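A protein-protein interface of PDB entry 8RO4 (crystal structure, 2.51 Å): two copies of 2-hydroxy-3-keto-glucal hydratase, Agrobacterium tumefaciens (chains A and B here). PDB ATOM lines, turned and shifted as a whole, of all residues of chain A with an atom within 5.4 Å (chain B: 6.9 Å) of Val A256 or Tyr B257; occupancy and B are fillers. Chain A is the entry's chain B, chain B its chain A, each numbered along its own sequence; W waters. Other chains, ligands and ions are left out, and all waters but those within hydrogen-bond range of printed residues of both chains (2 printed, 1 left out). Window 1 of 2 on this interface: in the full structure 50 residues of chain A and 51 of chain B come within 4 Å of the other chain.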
ATOM      1  N   TRP A 143      40.745  14.911  23.302  1.00  0.00           N
ATOM      2  CA  TRP A 143      39.533  14.877  22.485  1.00  0.00           C
ATOM      3  C   TRP A 143      39.786  14.799  20.980  1.00  0.00           C
ATOM      4  O   TRP A 143      39.015  14.103  20.297  1.00  0.00           O
ATOM      5  CB  TRP A 143      38.640  16.083  22.795  1.00  0.00           C
ATOM      6  CG  TRP A 143      37.393  16.058  21.962  1.00  0.00           C
ATOM      7  CD1 TRP A 143      37.132  16.808  20.854  1.00  0.00           C
ATOM      8  CD2 TRP A 143      36.249  15.215  22.154  1.00  0.00           C
ATOM      9  NE1 TRP A 143      35.893  16.491  20.349  1.00  0.00           N
ATOM     10  CE2 TRP A 143      35.330  15.517  21.130  1.00  0.00           C
ATOM     11  CE3 TRP A 143      35.911  14.239  23.098  1.00  0.00           C
ATOM     12  CZ2 TRP A 143      34.092  14.879  21.021  1.00  0.00           C
ATOM     13  CZ3 TRP A 143      34.680  13.606  22.990  1.00  0.00           C
ATOM     14  CH2 TRP A 143      33.787  13.929  21.958  1.00  0.00           C
ATOM     15  N   ILE A 146      39.604  11.100  19.687  1.00  0.00           N
ATOM     16  CA  ILE A 146      38.508  10.284  20.203  1.00  0.00           C
ATOM     17  C   ILE A 146      38.275   9.062  19.316  1.00  0.00           C
ATOM     18  O   ILE A 146      37.967   7.972  19.812  1.00  0.00           O
ATOM     19  CB  ILE A 146      37.235  11.144  20.360  1.00  0.00           C
ATOM     20  CG1 ILE A 146      36.136  10.366  21.089  1.00  0.00           C
ATOM     21  CG2 ILE A 146      36.737  11.663  19.006  1.00  0.00           C
ATOM     22  CD1 ILE A 146      36.501   9.971  22.502  1.00  0.00           C
ATOM     23  N   PRO A 188      30.457  16.011  25.670  1.00  0.00           N
ATOM     24  CA  PRO A 188      31.359  15.903  24.517  1.00  0.00           C
ATOM     25  C   PRO A 188      32.349  17.058  24.499  1.00  0.00           C
ATOM     26  O   PRO A 188      32.062  18.160  24.972  1.00  0.00           O
ATOM     27  CB  PRO A 188      30.412  15.962  23.312  1.00  0.00           C
ATOM     28  CG  PRO A 188      29.070  15.604  23.859  1.00  0.00           C
ATOM     29  CD  PRO A 188      29.046  16.109  25.264  1.00  0.00           C
ATOM     30  N   HIS A 193      33.571  12.197  29.269  1.00  0.00           N
ATOM     31  CA  HIS A 193      32.361  12.262  28.458  1.00  0.00           C
ATOM     32  C   HIS A 193      31.463  11.038  28.597  1.00  0.00           C
ATOM     33  O   HIS A 193      30.413  10.989  27.947  1.00  0.00           O
ATOM     34  CB  HIS A 193      32.711  12.473  26.976  1.00  0.00           C
ATOM     35  CG  HIS A 193      33.531  11.370  26.385  1.00  0.00           C
ATOM     36  ND1 HIS A 193      34.905  11.428  26.300  1.00  0.00           N
ATOM     37  CD2 HIS A 193      33.172  10.174  25.862  1.00  0.00           C
ATOM     38  CE1 HIS A 193      35.357  10.319  25.743  1.00  0.00           C
ATOM     39  NE2 HIS A 193      34.325   9.541  25.469  1.00  0.00           N
ATOM     40  N   LEU A 222      22.369  11.982  23.061  1.00  0.00           N
ATOM     41  CA  LEU A 222      22.988  12.433  21.819  1.00  0.00           C
ATOM     42  C   LEU A 222      24.072  11.486  21.319  1.00  0.00           C
ATOM     43  O   LEU A 222      24.470  11.592  20.156  1.00  0.00           O
ATOM     44  CB  LEU A 222      23.587  13.830  21.998  1.00  0.00           C
ATOM     45  CG  LEU A 222      22.624  15.020  22.023  1.00  0.00           C
ATOM     46  CD1 LEU A 222      23.329  16.275  21.526  1.00  0.00           C
ATOM     47  CD2 LEU A 222      21.368  14.746  21.220  1.00  0.00           C
ATOM     48  N   GLN A 223      24.562  10.570  22.157  1.00  0.00           N
ATOM     49  CA  GLN A 223      25.548   9.589  21.712  1.00  0.00           C
ATOM     50  C   GLN A 223      25.025   8.157  21.814  1.00  0.00           C
ATOM     51  O   GLN A 223      25.820   7.208  21.791  1.00  0.00           O
ATOM     52  CB  GLN A 223      26.860   9.740  22.488  1.00  0.00           C
ATOM     53  CG  GLN A 223      26.764   9.547  23.994  1.00  0.00           C
ATOM     54  CD  GLN A 223      28.127   9.620  24.665  1.00  0.00           C
ATOM     55  OE1 GLN A 223      29.042   8.875  24.314  1.00  0.00           O
ATOM     56  NE2 GLN A 223      28.269  10.522  25.631  1.00  0.00           N
ATOM     57  N   ALA A 224      23.704   7.986  21.911  1.00  0.00           N
ATOM     58  CA  ALA A 224      23.058   6.671  21.929  1.00  0.00           C
ATOM     59  C   ALA A 224      23.598   5.805  23.069  1.00  0.00           C
ATOM     60  O   ALA A 224      24.075   4.688  22.872  1.00  0.00           O
ATOM     61  CB  ALA A 224      23.214   5.966  20.574  1.00  0.00           C
ATOM     62  N   PHE A 248      17.179  12.077  19.440  1.00  0.00           N
ATOM     63  CA  PHE A 248      18.119  11.536  18.461  1.00  0.00           C
ATOM     64  C   PHE A 248      17.325  10.772  17.413  1.00  0.00           C
ATOM     65  O   PHE A 248      16.775   9.705  17.705  1.00  0.00           O
ATOM     66  CB  PHE A 248      19.166  10.639  19.125  1.00  0.00           C
ATOM     67  CG  PHE A 248      20.114  10.002  18.152  1.00  0.00           C
ATOM     68  CD1 PHE A 248      20.900  10.785  17.321  1.00  0.00           C
ATOM     69  CD2 PHE A 248      20.225   8.623  18.070  1.00  0.00           C
ATOM     70  CE1 PHE A 248      21.773  10.203  16.416  1.00  0.00           C
ATOM     71  CE2 PHE A 248      21.099   8.035  17.173  1.00  0.00           C
ATOM     72  CZ  PHE A 248      21.873   8.826  16.344  1.00  0.00           C
ATOM     73  N   SER A 254      22.747  11.096   8.050  1.00  0.00           N
ATOM     74  CA  SER A 254      23.607  11.525   9.143  1.00  0.00           C
ATOM     75  C   SER A 254      23.304  10.715  10.396  1.00  0.00           C
ATOM     76  O   SER A 254      22.209  10.170  10.560  1.00  0.00           O
ATOM     77  CB  SER A 254      23.448  13.024   9.416  1.00  0.00           C
ATOM     78  OG  SER A 254      24.467  13.482  10.285  1.00  0.00           O
ATOM     79  N   GLY A 255      24.293  10.658  11.286  1.00  0.00           N
ATOM     80  CA  GLY A 255      24.191   9.952  12.550  1.00  0.00           C
ATOM     81  C   GLY A 255      24.698  10.817  13.692  1.00  0.00           C
ATOM     82  O   GLY A 255      24.505  12.029  13.715  1.00  0.00           O
ATOM     83  N   VAL A 256      25.388  10.174  14.637  1.00  0.00           N
ATOM     84  CA  VAL A 256      25.796  10.858  15.863  1.00  0.00           C
ATOM     85  C   VAL A 256      26.799  11.969  15.563  1.00  0.00           C
ATOM     86  O   VAL A 256      26.768  13.036  16.188  1.00  0.00           O
ATOM     87  CB  VAL A 256      26.353   9.843  16.879  1.00  0.00           C
ATOM     88  CG1 VAL A 256      27.159  10.544  17.964  1.00  0.00           C
ATOM     89  CG2 VAL A 256      25.219   9.045  17.502  1.00  0.00           C
ATOM     90  N   TYR A 257      27.697  11.748  14.600  1.00  0.00           N
ATOM     91  CA  TYR A 257      28.724  12.749  14.315  1.00  0.00           C
ATOM     92  C   TYR A 257      28.112  14.057  13.823  1.00  0.00           C
ATOM     93  O   TYR A 257      28.582  15.140  14.188  1.00  0.00           O
ATOM     94  CB  TYR A 257      29.731  12.188  13.315  1.00  0.00           C
ATOM     95  CG  TYR A 257      30.507  11.022  13.883  1.00  0.00           C
ATOM     96  CD1 TYR A 257      30.989  11.063  15.187  1.00  0.00           C
ATOM     97  CD2 TYR A 257      30.751   9.878  13.130  1.00  0.00           C
ATOM     98  CE1 TYR A 257      31.696  10.005  15.726  1.00  0.00           C
ATOM     99  CE2 TYR A 257      31.460   8.809  13.663  1.00  0.00           C
ATOM    100  CZ  TYR A 257      31.929   8.881  14.962  1.00  0.00           C
ATOM    101  OH  TYR A 257      32.633   7.827  15.500  1.00  0.00           O
ATOM    102  N   GLY A 258      27.074  13.980  12.987  1.00  0.00           N
ATOM    103  CA  GLY A 258      26.250  15.129  12.670  1.00  0.00           C
ATOM    104  C   GLY A 258      26.583  15.849  11.379  1.00  0.00           C
ATOM    105  O   GLY A 258      25.769  16.661  10.919  1.00  0.00           O
ATOM    106  N   ARG A 266      20.625  18.766  12.848  1.00  0.00           N
ATOM    107  CA  ARG A 266      21.359  17.607  13.331  1.00  0.00           C
ATOM    108  C   ARG A 266      20.389  16.491  13.713  1.00  0.00           C
ATOM    109  O   ARG A 266      19.305  16.763  14.238  1.00  0.00           O
ATOM    110  CB  ARG A 266      22.214  17.981  14.539  1.00  0.00           C
ATOM    111  CG  ARG A 266      23.595  18.503  14.202  1.00  0.00           C
ATOM    112  CD  ARG A 266      24.265  19.020  15.458  1.00  0.00           C
ATOM    113  NE  ARG A 266      24.436  17.964  16.448  1.00  0.00           N
ATOM    114  CZ  ARG A 266      25.577  17.330  16.678  1.00  0.00           C
ATOM    115  NH1 ARG A 266      26.681  17.626  16.010  1.00  0.00           N
ATOM    116  NH2 ARG A 266      25.613  16.372  17.601  1.00  0.00           N
ATOM    117  N   ILE B 146      34.335  18.472  15.130  1.00  0.00           N
ATOM    118  CA  ILE B 146      33.135  17.729  14.756  1.00  0.00           C
ATOM    119  C   ILE B 146      31.995  18.017  15.728  1.00  0.00           C
ATOM    120  O   ILE B 146      30.827  18.083  15.329  1.00  0.00           O
ATOM    121  CB  ILE B 146      33.448  16.221  14.660  1.00  0.00           C
ATOM    122  CG1 ILE B 146      32.262  15.458  14.070  1.00  0.00           C
ATOM    123  CG2 ILE B 146      33.837  15.641  16.018  1.00  0.00           C
ATOM    124  CD1 ILE B 146      31.921  15.864  12.655  1.00  0.00           C
ATOM    125  N   TYR B 147      32.312  18.202  17.024  1.00  0.00           N
ATOM    126  CA  TYR B 147      31.246  18.573  17.949  1.00  0.00           C
ATOM    127  C   TYR B 147      31.290  20.069  18.213  1.00  0.00           C
ATOM    128  O   TYR B 147      32.376  20.610  18.463  1.00  0.00           O
ATOM    129  CB  TYR B 147      31.363  17.815  19.271  1.00  0.00           C
ATOM    130  CG  TYR B 147      30.161  18.040  20.154  1.00  0.00           C
ATOM    131  CD1 TYR B 147      28.988  17.324  19.952  1.00  0.00           C
ATOM    132  CD2 TYR B 147      30.176  19.006  21.154  1.00  0.00           C
ATOM    133  CE1 TYR B 147      27.874  17.540  20.737  1.00  0.00           C
ATOM    134  CE2 TYR B 147      29.066  19.231  21.945  1.00  0.00           C
ATOM    135  CZ  TYR B 147      27.917  18.494  21.733  1.00  0.00           C
ATOM    136  OH  TYR B 147      26.808  18.710  22.516  1.00  0.00           O
ATOM    137  N   ASP B 194      29.683  11.128   6.156  1.00  0.00           N
ATOM    138  CA  ASP B 194      28.292  10.705   6.016  1.00  0.00           C
ATOM    139  C   ASP B 194      27.736  11.303   4.726  1.00  0.00           C
ATOM    140  O   ASP B 194      28.476  11.873   3.916  1.00  0.00           O
ATOM    141  CB  ASP B 194      27.452  11.088   7.243  1.00  0.00           C
ATOM    142  CG  ASP B 194      27.425  12.587   7.507  1.00  0.00           C
ATOM    143  OD1 ASP B 194      27.968  13.369   6.697  1.00  0.00           O
ATOM    144  OD2 ASP B 194      26.832  12.985   8.535  1.00  0.00           O
ATOM    145  N   LEU B 222      28.575   1.961  13.116  1.00  0.00           N
ATOM    146  CA  LEU B 222      29.357   2.411  14.263  1.00  0.00           C
ATOM    147  C   LEU B 222      28.931   3.781  14.773  1.00  0.00           C
ATOM    148  O   LEU B 222      29.300   4.148  15.893  1.00  0.00           O
ATOM    149  CB  LEU B 222      30.845   2.438  13.911  1.00  0.00           C
ATOM    150  CG  LEU B 222      31.565   1.088  13.867  1.00  0.00           C
ATOM    151  CD1 LEU B 222      33.050   1.262  14.176  1.00  0.00           C
ATOM    152  CD2 LEU B 222      30.921   0.083  14.815  1.00  0.00           C
ATOM    153  N   GLN B 223      28.167   4.545  13.988  1.00  0.00           N
ATOM    154  CA  GLN B 223      27.657   5.836  14.437  1.00  0.00           C
ATOM    155  C   GLN B 223      26.131   5.863  14.488  1.00  0.00           C
ATOM    156  O   GLN B 223      25.534   6.945  14.494  1.00  0.00           O
ATOM    157  CB  GLN B 223      28.186   6.973  13.557  1.00  0.00           C
ATOM    158  CG  GLN B 223      27.809   6.897  12.091  1.00  0.00           C
ATOM    159  CD  GLN B 223      28.280   8.113  11.310  1.00  0.00           C
ATOM    160  OE1 GLN B 223      27.958   9.249  11.658  1.00  0.00           O
ATOM    161  NE2 GLN B 223      29.042   7.878  10.249  1.00  0.00           N
ATOM    162  N   ALA B 224      25.490   4.692  14.516  1.00  0.00           N
ATOM    163  CA  ALA B 224      24.037   4.563  14.659  1.00  0.00           C
ATOM    164  C   ALA B 224      23.300   5.321  13.550  1.00  0.00           C
ATOM    165  O   ALA B 224      22.441   6.168  13.797  1.00  0.00           O
ATOM    166  CB  ALA B 224      23.584   5.027  16.047  1.00  0.00           C
ATOM    167  N   MET B 225      23.649   4.983  12.313  1.00  0.00           N
ATOM    168  CA  MET B 225      23.087   5.607  11.124  1.00  0.00           C
ATOM    169  C   MET B 225      22.474   4.532  10.230  1.00  0.00           C
ATOM    170  O   MET B 225      22.986   3.410  10.158  1.00  0.00           O
ATOM    171  CB  MET B 225      24.181   6.402  10.407  1.00  0.00           C
ATOM    172  CG  MET B 225      23.822   7.024   9.086  1.00  0.00           C
ATOM    173  SD  MET B 225      25.270   7.916   8.482  1.00  0.00           S
ATOM    174  CE  MET B 225      24.875   8.068   6.741  1.00  0.00           C
ATOM    175  N   PHE B 248      26.995  -2.568  17.263  1.00  0.00           N
ATOM    176  CA  PHE B 248      26.923  -1.450  18.196  1.00  0.00           C
ATOM    177  C   PHE B 248      26.014  -1.859  19.346  1.00  0.00           C
ATOM    178  O   PHE B 248      24.797  -1.985  19.166  1.00  0.00           O
ATOM    179  CB  PHE B 248      26.411  -0.183  17.505  1.00  0.00           C
ATOM    180  CG  PHE B 248      26.226   0.981  18.432  1.00  0.00           C
ATOM    181  CD1 PHE B 248      27.295   1.486  19.155  1.00  0.00           C
ATOM    182  CD2 PHE B 248      24.980   1.566  18.588  1.00  0.00           C
ATOM    183  CE1 PHE B 248      27.123   2.558  20.020  1.00  0.00           C
ATOM    184  CE2 PHE B 248      24.799   2.637  19.447  1.00  0.00           C
ATOM    185  CZ  PHE B 248      25.872   3.134  20.164  1.00  0.00           C
ATOM    186  N   SER B 254      29.178   3.660  28.178  1.00  0.00           N
ATOM    187  CA  SER B 254      29.806   4.191  26.976  1.00  0.00           C
ATOM    188  C   SER B 254      28.815   4.145  25.824  1.00  0.00           C
ATOM    189  O   SER B 254      27.865   3.357  25.828  1.00  0.00           O
ATOM    190  CB  SER B 254      31.078   3.413  26.622  1.00  0.00           C
ATOM    191  OG  SER B 254      31.818   4.077  25.613  1.00  0.00           O
ATOM    192  N   GLY B 255      29.056   5.003  24.837  1.00  0.00           N
ATOM    193  CA  GLY B 255      28.239   5.102  23.643  1.00  0.00           C
ATOM    194  C   GLY B 255      29.108   5.143  22.399  1.00  0.00           C
ATOM    195  O   GLY B 255      30.129   4.464  22.299  1.00  0.00           O
ATOM    196  N   VAL B 256      28.688   5.972  21.437  1.00  0.00           N
ATOM    197  CA  VAL B 256      29.337   6.002  20.128  1.00  0.00           C
ATOM    198  C   VAL B 256      30.769   6.522  20.235  1.00  0.00           C
ATOM    199  O   VAL B 256      31.669   6.045  19.534  1.00  0.00           O
ATOM    200  CB  VAL B 256      28.492   6.832  19.139  1.00  0.00           C
ATOM    201  CG1 VAL B 256      29.317   7.248  17.928  1.00  0.00           C
ATOM    202  CG2 VAL B 256      27.279   6.028  18.687  1.00  0.00           C
ATOM    203  N   TYR B 257      31.008   7.502  21.110  1.00  0.00           N
ATOM    204  CA  TYR B 257      32.340   8.090  21.210  1.00  0.00           C
ATOM    205  C   TYR B 257      33.371   7.067  21.681  1.00  0.00           C
ATOM    206  O   TYR B 257      34.511   7.063  21.203  1.00  0.00           O
ATOM    207  CB  TYR B 257      32.299   9.309  22.127  1.00  0.00           C
ATOM    208  CG  TYR B 257      31.420  10.407  21.571  1.00  0.00           C
ATOM    209  CD1 TYR B 257      31.466  10.737  20.223  1.00  0.00           C
ATOM    210  CD2 TYR B 257      30.530  11.095  22.385  1.00  0.00           C
ATOM    211  CE1 TYR B 257      30.661  11.731  19.701  1.00  0.00           C
ATOM    212  CE2 TYR B 257      29.719  12.093  21.870  1.00  0.00           C
ATOM    213  CZ  TYR B 257      29.789  12.406  20.528  1.00  0.00           C
ATOM    214  OH  TYR B 257      28.983  13.398  20.013  1.00  0.00           O
ATOM    215  N   GLY B 258      32.994   6.198  22.618  1.00  0.00           N
ATOM    216  CA  GLY B 258      33.780   5.026  22.946  1.00  0.00           C
ATOM    217  C   GLY B 258      34.667   5.139  24.168  1.00  0.00           C
ATOM    218  O   GLY B 258      35.160   4.110  24.645  1.00  0.00           O
ATOM    219  N   GLY B 259      34.896   6.348  24.679  1.00  0.00           N
ATOM    220  CA  GLY B 259      35.665   6.506  25.899  1.00  0.00           C
ATOM    221  C   GLY B 259      37.121   6.103  25.805  1.00  0.00           C
ATOM    222  O   GLY B 259      37.686   5.620  26.792  1.00  0.00           O
ATOM    223  N   TYR B 260      37.747   6.298  24.642  1.00  0.00           N
ATOM    224  CA  TYR B 260      39.150   5.962  24.391  1.00  0.00           C
ATOM    225  C   TYR B 260      39.452   4.480  24.595  1.00  0.00           C
ATOM    226  O   TYR B 260      40.616   4.102  24.761  1.00  0.00           O
ATOM    227  CB  TYR B 260      40.096   6.806  25.259  1.00  0.00           C
ATOM    228  CG  TYR B 260      39.875   8.294  25.151  1.00  0.00           C
ATOM    229  CD1 TYR B 260      40.230   8.986  23.998  1.00  0.00           C
ATOM    230  CD2 TYR B 260      39.321   9.014  26.204  1.00  0.00           C
ATOM    231  CE1 TYR B 260      40.031  10.350  23.889  1.00  0.00           C
ATOM    232  CE2 TYR B 260      39.117  10.382  26.104  1.00  0.00           C
ATOM    233  CZ  TYR B 260      39.476  11.043  24.945  1.00  0.00           C
ATOM    234  OH  TYR B 260      39.278  12.400  24.837  1.00  0.00           O
ATOM    235  N   GLN B 261      38.437   3.623  24.576  1.00  0.00           N
ATOM    236  CA  GLN B 261      38.667   2.203  24.786  1.00  0.00           C
ATOM    237  C   GLN B 261      39.206   1.542  23.521  1.00  0.00           C
ATOM    238  O   GLN B 261      39.072   2.058  22.407  1.00  0.00           O
ATOM    239  CB  GLN B 261      37.381   1.504  25.231  1.00  0.00           C
ATOM    240  CG  GLN B 261      36.952   1.836  26.648  1.00  0.00           C
ATOM    241  CD  GLN B 261      35.638   1.180  27.023  1.00  0.00           C
ATOM    242  OE1 GLN B 261      34.616   1.392  26.370  1.00  0.00           O
ATOM    243  NE2 GLN B 261      35.659   0.370  28.077  1.00  0.00           N
ATOM    244  N   ARG B 266      35.045  -1.445  23.044  1.00  0.00           N
ATOM    245  CA  ARG B 266      34.173  -0.385  22.558  1.00  0.00           C
ATOM    246  C   ARG B 266      32.751  -0.908  22.372  1.00  0.00           C
ATOM    247  O   ARG B 266      32.559  -2.066  21.987  1.00  0.00           O
ATOM    248  CB  ARG B 266      34.686   0.176  21.234  1.00  0.00           C
ATOM    249  CG  ARG B 266      35.673   1.320  21.364  1.00  0.00           C
ATOM    250  CD  ARG B 266      36.256   1.654  20.004  1.00  0.00           C
ATOM    251  NE  ARG B 266      35.222   2.081  19.070  1.00  0.00           N
ATOM    252  CZ  ARG B 266      34.980   3.342  18.742  1.00  0.00           C
ATOM    253  NH1 ARG B 266      35.691   4.336  19.247  1.00  0.00           N
ATOM    254  NH2 ARG B 266      34.000   3.612  17.884  1.00  0.00           N
ATOM    255  N   PRO B 267      31.736  -0.087  22.647  1.00  0.00           N
ATOM    256  CA  PRO B 267      30.365  -0.504  22.310  1.00  0.00           C
ATOM    257  C   PRO B 267      30.194  -0.782  20.827  1.00  0.00           C
ATOM    258  O   PRO B 267      29.515  -1.746  20.453  1.00  0.00           O
ATOM    259  CB  PRO B 267      29.513   0.686  22.775  1.00  0.00           C
ATOM    260  CG  PRO B 267      30.343   1.363  23.814  1.00  0.00           C
ATOM    261  CD  PRO B 267      31.765   1.203  23.357  1.00  0.00           C
HETATM  262  O   HOH W   1      36.857   6.676  22.004  1.00  0.00           O
HETATM  263  O   HOH W   2      28.999  17.549  13.366  1.00  0.00           O
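Among the printed residues, pairs that only touch across the chains: Ile A146 with Tyr B257 (3.7 Å), Ile A146 with Tyr B260 (3.8 Å), Pro A188 with Tyr B147 (3.7 Å), His A193 with Tyr B257 (3.9 Å), His A193 with Tyr B260 (3.8 Å), Gln A223 with Gly B255 (3.7 Å), Gln A223 with Tyr B257 (3.3 Å), Ala A224 with Phe B248 (3.6 Å), Phe A248 with Ala B224 (3.7 Å), Ser A254 with Met B225 (3.8 Å), Gly A255 with Gln B223 (3.8 Å), Val A256 with Val B256 (3.8 Å), Val A256 with Tyr B257 (3.96 Å), Tyr A257 with Ile B146 (3.7 Å) and Tyr A257 with Gln B223 (3.2 Å).
Water W1 lies within hydrogen-bond range of O of Tyr B257 (2.5 Å), O of Ile A146 (2.8 Å), N of Tyr B260 (2.8 Å) and N of Gly B259 (3.3 Å). Water W2 lies within hydrogen-bond range of O of Tyr A257 and O of Ile B146.
Gln A223 touches Val B256, and with the chains exchanged Val A256 touches Gln B223. Gln A223 touches Tyr B257, and with the chains exchanged Tyr A257 touches Gln B223. Val B256 touches its own counterpart, Val A256. Val A256 touches Tyr B257, but with the chains exchanged Tyr A257 does not touch Val B256 (4.2 Å). Of the 20 pairs that touch across the chains among the printed residues, 11 have their exchanged pair printed and touching as well.
O of His A193 sits at hydrogen-bond distance from NE2 of Gln A223 (3.2 Å). O of Gly A258 sits close to OG of Ser A254, 3.5 Å away.
The side-chain hydroxyl (OG) of Ser A254 sits at hydrogen-bond distance from the side-chain carboxylate (OD2) of Asp B194, at 3.0 Å. O of Gln B223 sits at hydrogen-bond distance from N of Val A256 (3.2 Å). The backbone NH (N) of Val B256 lies within hydrogen-bond range of the backbone carbonyl oxygen (O) of Gln A223, at 3.1 Å. A ring nitrogen (NE2) of His A193 lies within hydrogen-bond range of the backbone NH of Gly B259 (3.3 Å). The backbone NH (N) of Trp A143 lies within hydrogen-bond range of the side-chain hydroxyl (OH) of Tyr B260.
Of chain B, only Gln B223, Val B256 and Tyr B257 come within 4 Å of Val A256. Of chain A, only Ile A146, His A193, Gln A223 and Val A256 come within 4 Å of Tyr B257. Of the printed residues of chain A, Ile B146 touches Tyr A257 (3.7 Å). Of the printed residues of chain A, Gly B255 touches Gln A223 (3.7 Å). Of the printed residues of chain B, Gly A255 touches Gln B223 (3.8 Å). Printed residues of chain A within 4 Å of Gln B223: Gly A255, Val A256 and Tyr A257. Of the printed residues of chain B, Ser A254 touches Asp B194 and Met B225. Gln B261 touches none of the printed residues of chain A. Ser B254 touches none of the printed residues of chain A. The nearest printed residue of chain B that does not touch His A193 is Gly B258 (4.6 Å).
Hydrophobic or aromatic side chains of chain B that line the printed part of chain A: Ile B146, Tyr B147, Met B225, Phe B248, Val B256, Tyr B257 and Tyr B260. Of the 14 printed residues of chain A, 11 touch a printed residue of chain B. Hydrophobic or aromatic side chains of chain A within 4 Å of the printed part of chain B: Ile A146, Pro A188, His A193, Ala A224, Phe A248, Val A256 and Tyr A257. Along chain A the printed residues that touch a printed residue of chain B span positions 143 to 257. Among the printed residues, 20 pairs touch across the chains. Among the printed residues, no Asp or Glu carboxylate lies within 4 Å of a Lys or Arg side-chain nitrogen of the other chain.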
